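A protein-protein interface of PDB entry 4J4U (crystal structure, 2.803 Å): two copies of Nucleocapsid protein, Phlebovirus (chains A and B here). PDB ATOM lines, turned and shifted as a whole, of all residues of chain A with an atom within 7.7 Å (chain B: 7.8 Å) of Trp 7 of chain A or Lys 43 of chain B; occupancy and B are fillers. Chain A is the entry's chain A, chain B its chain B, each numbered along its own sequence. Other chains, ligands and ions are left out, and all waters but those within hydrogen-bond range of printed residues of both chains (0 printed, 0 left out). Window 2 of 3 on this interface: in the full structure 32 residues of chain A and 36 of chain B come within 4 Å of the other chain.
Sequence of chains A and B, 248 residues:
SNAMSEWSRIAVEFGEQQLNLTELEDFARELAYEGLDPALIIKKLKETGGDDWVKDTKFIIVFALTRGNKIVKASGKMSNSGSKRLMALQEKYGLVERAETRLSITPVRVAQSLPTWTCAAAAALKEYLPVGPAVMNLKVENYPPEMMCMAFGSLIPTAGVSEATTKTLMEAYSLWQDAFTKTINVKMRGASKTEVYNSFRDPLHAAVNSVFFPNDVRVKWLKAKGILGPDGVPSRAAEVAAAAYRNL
The side-chain hydroxyl (OG) of Ser 8 of chain A is in hydrogen-bond range of the backbone carbonyl oxygen (O) of Phe 212 of chain B, 2.6 Å away. The side-chain sulfur (SD) of Met 4 of chain A lies close to the backbone carbonyl oxygen (O) of Phe 212 of chain B.
The backbone NH of Ala 3 of chain A sits at hydrogen-bond distance from the side-chain hydroxyl of Ser 8 of chain A (3.4 Å). OG of Ser 5 of chain A lies within hydrogen-bond range of N of Ser 8 of chain A (3.1 Å). NZ of Lys 43 of chain B lies within salt-bridge range of OE1 of Glu 47 of chain B, at 2.7 Å.
CH2 of Trp 7 of chain A touches CG of Lys 43 of chain B (3.4 Å). Trp 7 of chain A touches Phe 212 of chain B. CG2 of Ile 10 of chain A touches CG2 of Ile 42 of chain B (3.9 Å). CH2 of Trp 53 of chain B touches CG2 of Ile 10 of chain A, 3.8 Å away. Ile 42 of chain B touches Ala 11 of chain A. Ser 113 of chain B touches Ala 11 of chain A. CA of Ala 11 of chain A touches CD1 of Leu 114 of chain B, at 3.8 Å. CB of Ala 11 of chain A touches CE2 of Phe 212 of chain B, 3.8 Å away. CE2 of Phe 213 of chain B touches CB of Ala 11 of chain A, 3.8 Å away. Phe 213 of chain B touches Val 12 of chain A.
Trp 7 of chain A touches two residues of chain B. Printed residues of chain B within 4 Å of Ala 11 of chain A: Ile 42 (3.98 Å), Ser 113 (3.9 Å), Leu 114 (3.8 Å), Phe 212 (3.8 Å) and Phe 213 (3.8 Å). Lys 43 of chain B touches just one residue of chain A: Trp 7. Lys 44 of chain B touches none of the printed residues of chain A. Of the printed residues of chain A, Leu 114 of chain B touches Ala 11 (3.8 Å). Of the printed residues of chain A, Phe 213 of chain B touches Ala 11 (3.8 Å) and Val 12 (3.95 Å). The nearest printed residue of chain B that does not touch Trp 7 of chain A is Ala 39 of chain B (4.03 Å). The nearest residue of chain A that does not touch Lys 43 of chain B is Ile 10 of chain A (6.7 Å).
Of the 11 printed residues of chain A, 6 touch a printed residue of chain B. Printed residues of chain A that touch a printed residue of chain B: Met 4, Trp 7, Ser 8, Ile 10, Ala 11 and Val 12. Among the printed residues, no Asp or Glu carboxylate lies within 4 Å of a Lys or Arg side-chain nitrogen of the other chain.
No position is printed for both chains.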
ATOM      1  N   ALA A   3     -29.030  17.750  19.416  1.00  0.00           N
ATOM      2  CA  ALA A   3     -29.189  17.251  20.775  1.00  0.00           C
ATOM      3  C   ALA A   3     -27.854  17.183  21.518  1.00  0.00           C
ATOM      4  O   ALA A   3     -27.725  17.703  22.626  1.00  0.00           O
ATOM      5  CB  ALA A   3     -29.873  15.886  20.771  1.00  0.00           C
ATOM      6  N   MET A   4     -26.858  16.558  20.897  1.00  0.00           N
ATOM      7  CA  MET A   4     -25.599  16.249  21.579  1.00  0.00           C
ATOM      8  C   MET A   4     -24.780  17.467  22.027  1.00  0.00           C
ATOM      9  O   MET A   4     -24.244  17.487  23.136  1.00  0.00           O
ATOM     10  CB  MET A   4     -24.742  15.300  20.732  1.00  0.00           C
ATOM     11  CG  MET A   4     -24.426  15.801  19.337  1.00  0.00           C
ATOM     12  SD  MET A   4     -23.888  14.448  18.290  1.00  0.00           S
ATOM     13  CE  MET A   4     -25.017  13.167  18.856  1.00  0.00           C
ATOM     14  N   SER A   5     -24.666  18.473  21.174  1.00  0.00           N
ATOM     15  CA  SER A   5     -23.964  19.680  21.566  1.00  0.00           C
ATOM     16  C   SER A   5     -24.906  20.844  21.394  1.00  0.00           C
ATOM     17  O   SER A   5     -26.048  20.663  20.992  1.00  0.00           O
ATOM     18  CB  SER A   5     -22.712  19.878  20.718  1.00  0.00           C
ATOM     19  OG  SER A   5     -23.005  19.691  19.345  1.00  0.00           O
ATOM     20  N   GLU A   6     -24.433  22.043  21.696  1.00  0.00           N
ATOM     21  CA  GLU A   6     -25.227  23.231  21.443  1.00  0.00           C
ATOM     22  C   GLU A   6     -25.315  23.440  19.940  1.00  0.00           C
ATOM     23  O   GLU A   6     -26.292  23.980  19.421  1.00  0.00           O
ATOM     24  CB  GLU A   6     -24.606  24.455  22.123  1.00  0.00           C
ATOM     25  CG  GLU A   6     -23.107  24.584  21.910  1.00  0.00           C
ATOM     26  CD  GLU A   6     -22.538  25.879  22.460  1.00  0.00           C
ATOM     27  OE1 GLU A   6     -21.482  25.804  23.146  1.00  0.00           O
ATOM     28  OE2 GLU A   6     -23.144  26.955  22.194  1.00  0.00           O
ATOM     29  N   TRP A   7     -24.280  22.997  19.240  1.00  0.00           N
ATOM     30  CA  TRP A   7     -24.255  23.092  17.790  1.00  0.00           C
ATOM     31  C   TRP A   7     -25.266  22.133  17.180  1.00  0.00           C
ATOM     32  O   TRP A   7     -26.035  22.502  16.296  1.00  0.00           O
ATOM     33  CB  TRP A   7     -22.847  22.828  17.282  1.00  0.00           C
ATOM     34  CG  TRP A   7     -21.833  23.609  18.063  1.00  0.00           C
ATOM     35  CD1 TRP A   7     -20.827  23.104  18.831  1.00  0.00           C
ATOM     36  CD2 TRP A   7     -21.754  25.040  18.186  1.00  0.00           C
ATOM     37  NE1 TRP A   7     -20.111  24.127  19.403  1.00  0.00           N
ATOM     38  CE2 TRP A   7     -20.660  25.325  19.026  1.00  0.00           C
ATOM     39  CE3 TRP A   7     -22.493  26.106  17.658  1.00  0.00           C
ATOM     40  CZ2 TRP A   7     -20.288  26.631  19.351  1.00  0.00           C
ATOM     41  CZ3 TRP A   7     -22.121  27.402  17.984  1.00  0.00           C
ATOM     42  CH2 TRP A   7     -21.028  27.651  18.821  1.00  0.00           C
ATOM     43  N   SER A   8     -25.274  20.906  17.686  1.00  0.00           N
ATOM     44  CA  SER A   8     -26.286  19.927  17.321  1.00  0.00           C
ATOM     45  C   SER A   8     -27.719  20.448  17.554  1.00  0.00           C
ATOM     46  O   SER A   8     -28.576  20.363  16.666  1.00  0.00           O
ATOM     47  CB  SER A   8     -26.050  18.634  18.097  1.00  0.00           C
ATOM     48  OG  SER A   8     -26.407  17.504  17.329  1.00  0.00           O
ATOM     49  N   ARG A   9     -27.981  20.991  18.738  1.00  0.00           N
ATOM     50  CA  ARG A   9     -29.302  21.550  19.004  1.00  0.00           C
ATOM     51  C   ARG A   9     -29.659  22.727  18.091  1.00  0.00           C
ATOM     52  O   ARG A   9     -30.794  22.819  17.629  1.00  0.00           O
ATOM     53  CB  ARG A   9     -29.461  21.935  20.470  1.00  0.00           C
ATOM     54  CG  ARG A   9     -29.852  20.769  21.371  1.00  0.00           C
ATOM     55  CD  ARG A   9     -29.995  21.195  22.830  1.00  0.00           C
ATOM     56  NE  ARG A   9     -28.748  21.740  23.357  1.00  0.00           N
ATOM     57  CZ  ARG A   9     -28.482  23.039  23.486  1.00  0.00           C
ATOM     58  NH1 ARG A   9     -29.386  23.950  23.139  1.00  0.00           N
ATOM     59  NH2 ARG A   9     -27.309  23.426  23.972  1.00  0.00           N
ATOM     60  N   ILE A  10     -28.701  23.614  17.820  1.00  0.00           N
ATOM     61  CA  ILE A  10     -28.957  24.727  16.902  1.00  0.00           C
ATOM     62  C   ILE A  10     -29.408  24.226  15.523  1.00  0.00           C
ATOM     63  O   ILE A  10     -30.400  24.717  14.984  1.00  0.00           O
ATOM     64  CB  ILE A  10     -27.753  25.690  16.770  1.00  0.00           C
ATOM     65  CG1 ILE A  10     -27.530  26.469  18.069  1.00  0.00           C
ATOM     66  CG2 ILE A  10     -27.972  26.685  15.640  1.00  0.00           C
ATOM     67  CD1 ILE A  10     -26.361  27.465  17.993  1.00  0.00           C
ATOM     68  N   ALA A  11     -28.695  23.242  14.971  1.00  0.00           N
ATOM     69  CA  ALA A  11     -29.086  22.606  13.706  1.00  0.00           C
ATOM     70  C   ALA A  11     -30.526  22.086  13.730  1.00  0.00           C
ATOM     71  O   ALA A  11     -31.301  22.328  12.806  1.00  0.00           O
ATOM     72  CB  ALA A  11     -28.129  21.475  13.348  1.00  0.00           C
ATOM     73  N   VAL A  12     -30.878  21.378  14.796  1.00  0.00           N
ATOM     74  CA  VAL A  12     -32.225  20.851  14.942  1.00  0.00           C
ATOM     75  C   VAL A  12     -33.297  21.957  15.006  1.00  0.00           C
ATOM     76  O   VAL A  12     -34.253  21.918  14.232  1.00  0.00           O
ATOM     77  CB  VAL A  12     -32.319  19.899  16.140  1.00  0.00           C
ATOM     78  CG1 VAL A  12     -33.757  19.482  16.377  1.00  0.00           C
ATOM     79  CG2 VAL A  12     -31.440  18.680  15.899  1.00  0.00           C
ATOM     80  N   GLU A  13     -33.121  22.944  15.897  1.00  0.00           N
ATOM     81  CA  GLU A  13     -34.019  24.120  15.983  1.00  0.00           C
ATOM     82  C   GLU A  13     -34.130  24.944  14.674  1.00  0.00           C
ATOM     83  O   GLU A  13     -35.221  25.357  14.296  1.00  0.00           O
ATOM     84  CB  GLU A  13     -33.661  25.044  17.172  1.00  0.00           C
ATOM     85  CG  GLU A  13     -33.902  24.473  18.588  1.00  0.00           C
ATOM     86  CD  GLU A  13     -35.380  24.231  18.934  1.00  0.00           C
ATOM     87  OE1 GLU A  13     -36.211  25.159  18.758  1.00  0.00           O
ATOM     88  OE2 GLU A  13     -35.707  23.106  19.394  1.00  0.00           O
ATOM     89  N   ASP B  37     -17.185  19.558   8.883  1.00  0.00           N
ATOM     90  CA  ASP B  37     -17.461  19.806  10.300  1.00  0.00           C
ATOM     91  C   ASP B  37     -18.633  20.778  10.382  1.00  0.00           C
ATOM     92  O   ASP B  37     -18.457  21.981  10.248  1.00  0.00           O
ATOM     93  CB  ASP B  37     -16.244  20.385  11.038  1.00  0.00           C
ATOM     94  CG  ASP B  37     -16.384  20.298  12.560  1.00  0.00           C
ATOM     95  OD1 ASP B  37     -17.517  20.045  13.034  1.00  0.00           O
ATOM     96  OD2 ASP B  37     -15.373  20.483  13.285  1.00  0.00           O
ATOM     97  N   PRO B  38     -19.843  20.254  10.578  1.00  0.00           N
ATOM     98  CA  PRO B  38     -20.972  21.175  10.635  1.00  0.00           C
ATOM     99  C   PRO B  38     -20.896  22.063  11.881  1.00  0.00           C
ATOM    100  O   PRO B  38     -21.265  23.233  11.817  1.00  0.00           O
ATOM    101  CB  PRO B  38     -22.176  20.236  10.692  1.00  0.00           C
ATOM    102  CG  PRO B  38     -21.641  18.991  11.302  1.00  0.00           C
ATOM    103  CD  PRO B  38     -20.257  18.856  10.777  1.00  0.00           C
ATOM    104  N   ALA B  39     -20.409  21.510  12.985  1.00  0.00           N
ATOM    105  CA  ALA B  39     -20.270  22.259  14.227  1.00  0.00           C
ATOM    106  C   ALA B  39     -19.436  23.513  14.000  1.00  0.00           C
ATOM    107  O   ALA B  39     -19.891  24.630  14.287  1.00  0.00           O
ATOM    108  CB  ALA B  39     -19.641  21.393  15.298  1.00  0.00           C
ATOM    109  N   LEU B  40     -18.227  23.333  13.470  1.00  0.00           N
ATOM    110  CA  LEU B  40     -17.366  24.466  13.161  1.00  0.00           C
ATOM    111  C   LEU B  40     -18.019  25.476  12.213  1.00  0.00           C
ATOM    112  O   LEU B  40     -17.835  26.682  12.369  1.00  0.00           O
ATOM    113  CB  LEU B  40     -15.983  24.011  12.672  1.00  0.00           C
ATOM    114  CG  LEU B  40     -15.495  23.969  11.221  1.00  0.00           C
ATOM    115  CD1 LEU B  40     -15.353  25.324  10.578  1.00  0.00           C
ATOM    116  CD2 LEU B  40     -14.140  23.299  11.217  1.00  0.00           C
ATOM    117  N   ILE B  41     -18.787  24.987  11.245  1.00  0.00           N
ATOM    118  CA  ILE B  41     -19.465  25.863  10.288  1.00  0.00           C
ATOM    119  C   ILE B  41     -20.537  26.743  10.934  1.00  0.00           C
ATOM    120  O   ILE B  41     -20.539  27.954  10.744  1.00  0.00           O
ATOM    121  CB  ILE B  41     -20.053  25.056   9.141  1.00  0.00           C
ATOM    122  CG1 ILE B  41     -18.911  24.540   8.259  1.00  0.00           C
ATOM    123  CG2 ILE B  41     -21.051  25.881   8.338  1.00  0.00           C
ATOM    124  CD1 ILE B  41     -19.327  23.454   7.253  1.00  0.00           C
ATOM    125  N   ILE B  42     -21.432  26.128  11.700  1.00  0.00           N
ATOM    126  CA  ILE B  42     -22.465  26.851  12.442  1.00  0.00           C
ATOM    127  C   ILE B  42     -21.872  27.855  13.435  1.00  0.00           C
ATOM    128  O   ILE B  42     -22.300  29.015  13.498  1.00  0.00           O
ATOM    129  CB  ILE B  42     -23.405  25.870  13.163  1.00  0.00           C
ATOM    130  CG1 ILE B  42     -24.163  25.049  12.108  1.00  0.00           C
ATOM    131  CG2 ILE B  42     -24.364  26.615  14.092  1.00  0.00           C
ATOM    132  CD1 ILE B  42     -25.140  24.012  12.649  1.00  0.00           C
ATOM    133  N   LYS B  43     -20.878  27.407  14.192  1.00  0.00           N
ATOM    134  CA  LYS B  43     -20.209  28.278  15.149  1.00  0.00           C
ATOM    135  C   LYS B  43     -19.631  29.511  14.468  1.00  0.00           C
ATOM    136  O   LYS B  43     -19.805  30.624  14.937  1.00  0.00           O
ATOM    137  CB  LYS B  43     -19.109  27.516  15.883  1.00  0.00           C
ATOM    138  CG  LYS B  43     -18.299  28.356  16.835  1.00  0.00           C
ATOM    139  CD  LYS B  43     -17.077  27.577  17.282  1.00  0.00           C
ATOM    140  CE  LYS B  43     -15.992  28.469  17.867  1.00  0.00           C
ATOM    141  NZ  LYS B  43     -16.359  28.937  19.226  1.00  0.00           N
ATOM    142  N   LYS B  44     -18.948  29.310  13.351  1.00  0.00           N
ATOM    143  CA  LYS B  44     -18.415  30.437  12.596  1.00  0.00           C
ATOM    144  C   LYS B  44     -19.502  31.438  12.130  1.00  0.00           C
ATOM    145  O   LYS B  44     -19.399  32.633  12.389  1.00  0.00           O
ATOM    146  CB  LYS B  44     -17.551  29.946  11.434  1.00  0.00           C
ATOM    147  CG  LYS B  44     -17.045  31.061  10.549  1.00  0.00           C
ATOM    148  CD  LYS B  44     -15.886  31.821  11.185  1.00  0.00           C
ATOM    149  CE  LYS B  44     -15.605  33.133  10.464  1.00  0.00           C
ATOM    150  NZ  LYS B  44     -14.294  33.677  10.890  1.00  0.00           N
ATOM    151  N   LEU B  45     -20.550  30.944  11.479  1.00  0.00           N
ATOM    152  CA  LEU B  45     -21.637  31.794  10.981  1.00  0.00           C
ATOM    153  C   LEU B  45     -22.349  32.584  12.070  1.00  0.00           C
ATOM    154  O   LEU B  45     -22.679  33.747  11.877  1.00  0.00           O
ATOM    155  CB  LEU B  45     -22.678  30.956  10.241  1.00  0.00           C
ATOM    156  CG  LEU B  45     -22.218  30.226   8.984  1.00  0.00           C
ATOM    157  CD1 LEU B  45     -23.284  29.225   8.571  1.00  0.00           C
ATOM    158  CD2 LEU B  45     -21.909  31.209   7.865  1.00  0.00           C
ATOM    159  N   LYS B  46     -22.600  31.943  13.203  1.00  0.00           N
ATOM    160  CA  LYS B  46     -23.275  32.603  14.318  1.00  0.00           C
ATOM    161  C   LYS B  46     -22.393  33.667  14.963  1.00  0.00           C
ATOM    162  O   LYS B  46     -22.822  34.798  15.170  1.00  0.00           O
ATOM    163  CB  LYS B  46     -23.703  31.570  15.358  1.00  0.00           C
ATOM    164  CG  LYS B  46     -24.490  32.111  16.545  1.00  0.00           C
ATOM    165  CD  LYS B  46     -24.382  31.119  17.695  1.00  0.00           C
ATOM    166  CE  LYS B  46     -25.075  31.617  18.931  1.00  0.00           C
ATOM    167  NZ  LYS B  46     -26.511  31.832  18.638  1.00  0.00           N
ATOM    168  N   GLU B  47     -21.158  33.302  15.279  1.00  0.00           N
ATOM    169  CA  GLU B  47     -20.224  34.246  15.877  1.00  0.00           C
ATOM    170  C   GLU B  47     -19.913  35.429  14.965  1.00  0.00           C
ATOM    171  O   GLU B  47     -19.573  36.509  15.437  1.00  0.00           O
ATOM    172  CB  GLU B  47     -18.922  33.557  16.285  1.00  0.00           C
ATOM    173  CG  GLU B  47     -19.057  32.595  17.450  1.00  0.00           C
ATOM    174  CD  GLU B  47     -17.719  31.987  17.867  1.00  0.00           C
ATOM    175  OE1 GLU B  47     -17.695  31.245  18.877  1.00  0.00           O
ATOM    176  OE2 GLU B  47     -16.699  32.249  17.185  1.00  0.00           O
ATOM    177  N   THR B  48     -20.028  35.229  13.660  1.00  0.00           N
ATOM    178  CA  THR B  48     -19.673  36.281  12.721  1.00  0.00           C
ATOM    179  C   THR B  48     -20.899  37.135  12.412  1.00  0.00           C
ATOM    180  O   THR B  48     -20.822  38.360  12.273  1.00  0.00           O
ATOM    181  CB  THR B  48     -19.144  35.682  11.415  1.00  0.00           C
ATOM    182  OG1 THR B  48     -18.059  34.800  11.701  1.00  0.00           O
ATOM    183  CG2 THR B  48     -18.676  36.768  10.461  1.00  0.00           C
ATOM    184  N   GLY B  49     -22.037  36.477  12.325  1.00  0.00           N
ATOM    185  CA  GLY B  49     -23.196  37.121  11.776  1.00  0.00           C
ATOM    186  C   GLY B  49     -23.980  37.821  12.841  1.00  0.00           C
ATOM    187  O   GLY B  49     -24.627  38.830  12.582  1.00  0.00           O
ATOM    188  N   TRP B  53     -27.223  36.264  11.053  1.00  0.00           N
ATOM    189  CA  TRP B  53     -26.765  34.950  10.589  1.00  0.00           C
ATOM    190  C   TRP B  53     -27.886  34.010  10.153  1.00  0.00           C
ATOM    191  O   TRP B  53     -27.763  33.335   9.131  1.00  0.00           O
ATOM    192  CB  TRP B  53     -25.831  34.275  11.601  1.00  0.00           C
ATOM    193  CG  TRP B  53     -26.480  33.360  12.598  1.00  0.00           C
ATOM    194  CD1 TRP B  53     -26.964  33.705  13.820  1.00  0.00           C
ATOM    195  CD2 TRP B  53     -26.672  31.937  12.483  1.00  0.00           C
ATOM    196  NE1 TRP B  53     -27.459  32.601  14.477  1.00  0.00           N
ATOM    197  CE2 TRP B  53     -27.290  31.503  13.681  1.00  0.00           C
ATOM    198  CE3 TRP B  53     -26.388  30.993  11.488  1.00  0.00           C
ATOM    199  CZ2 TRP B  53     -27.634  30.175  13.910  1.00  0.00           C
ATOM    200  CZ3 TRP B  53     -26.734  29.656  11.717  1.00  0.00           C
ATOM    201  CH2 TRP B  53     -27.351  29.263  12.920  1.00  0.00           C
ATOM    202  N   SER B 113     -24.998  21.722   6.676  1.00  0.00           N
ATOM    203  CA  SER B 113     -24.925  21.835   8.130  1.00  0.00           C
ATOM    204  C   SER B 113     -26.238  22.268   8.790  1.00  0.00           C
ATOM    205  O   SER B 113     -26.332  22.323  10.012  1.00  0.00           O
ATOM    206  CB  SER B 113     -23.779  22.750   8.545  1.00  0.00           C
ATOM    207  OG  SER B 113     -22.534  22.205   8.160  1.00  0.00           O
ATOM    208  N   LEU B 114     -27.243  22.571   7.977  1.00  0.00           N
ATOM    209  CA  LEU B 114     -28.602  22.789   8.460  1.00  0.00           C
ATOM    210  C   LEU B 114     -29.602  21.940   7.641  1.00  0.00           C
ATOM    211  O   LEU B 114     -30.469  22.486   6.942  1.00  0.00           O
ATOM    212  CB  LEU B 114     -28.973  24.275   8.376  1.00  0.00           C
ATOM    213  CG  LEU B 114     -28.361  25.319   9.322  1.00  0.00           C
ATOM    214  CD1 LEU B 114     -28.320  24.848  10.768  1.00  0.00           C
ATOM    215  CD2 LEU B 114     -26.992  25.780   8.872  1.00  0.00           C
ATOM    216  N   PHE B 212     -23.450  13.838  14.246  1.00  0.00           N
ATOM    217  CA  PHE B 212     -23.843  15.210  14.539  1.00  0.00           C
ATOM    218  C   PHE B 212     -25.351  15.381  14.587  1.00  0.00           C
ATOM    219  O   PHE B 212     -25.912  15.584  15.655  1.00  0.00           O
ATOM    220  CB  PHE B 212     -23.249  16.158  13.497  1.00  0.00           C
ATOM    221  CG  PHE B 212     -23.681  17.591  13.653  1.00  0.00           C
ATOM    222  CD1 PHE B 212     -23.233  18.350  14.717  1.00  0.00           C
ATOM    223  CD2 PHE B 212     -24.528  18.184  12.720  1.00  0.00           C
ATOM    224  CE1 PHE B 212     -23.629  19.669  14.848  1.00  0.00           C
ATOM    225  CE2 PHE B 212     -24.924  19.513  12.847  1.00  0.00           C
ATOM    226  CZ  PHE B 212     -24.477  20.245  13.904  1.00  0.00           C
ATOM    227  N   PHE B 213     -26.008  15.290  13.435  1.00  0.00           N
ATOM    228  CA  PHE B 213     -27.464  15.422  13.374  1.00  0.00           C
ATOM    229  C   PHE B 213     -28.116  14.107  13.761  1.00  0.00           C
ATOM    230  O   PHE B 213     -28.010  13.130  13.028  1.00  0.00           O
ATOM    231  CB  PHE B 213     -27.888  15.809  11.974  1.00  0.00           C
ATOM    232  CG  PHE B 213     -29.149  16.591  11.927  1.00  0.00           C
ATOM    233  CD1 PHE B 213     -30.367  15.951  11.790  1.00  0.00           C
ATOM    234  CD2 PHE B 213     -29.121  17.972  12.004  1.00  0.00           C
ATOM    235  CE1 PHE B 213     -31.537  16.671  11.735  1.00  0.00           C
ATOM    236  CE2 PHE B 213     -30.291  18.700  11.948  1.00  0.00           C
ATOM    237  CZ  PHE B 213     -31.498  18.048  11.814  1.00  0.00           C
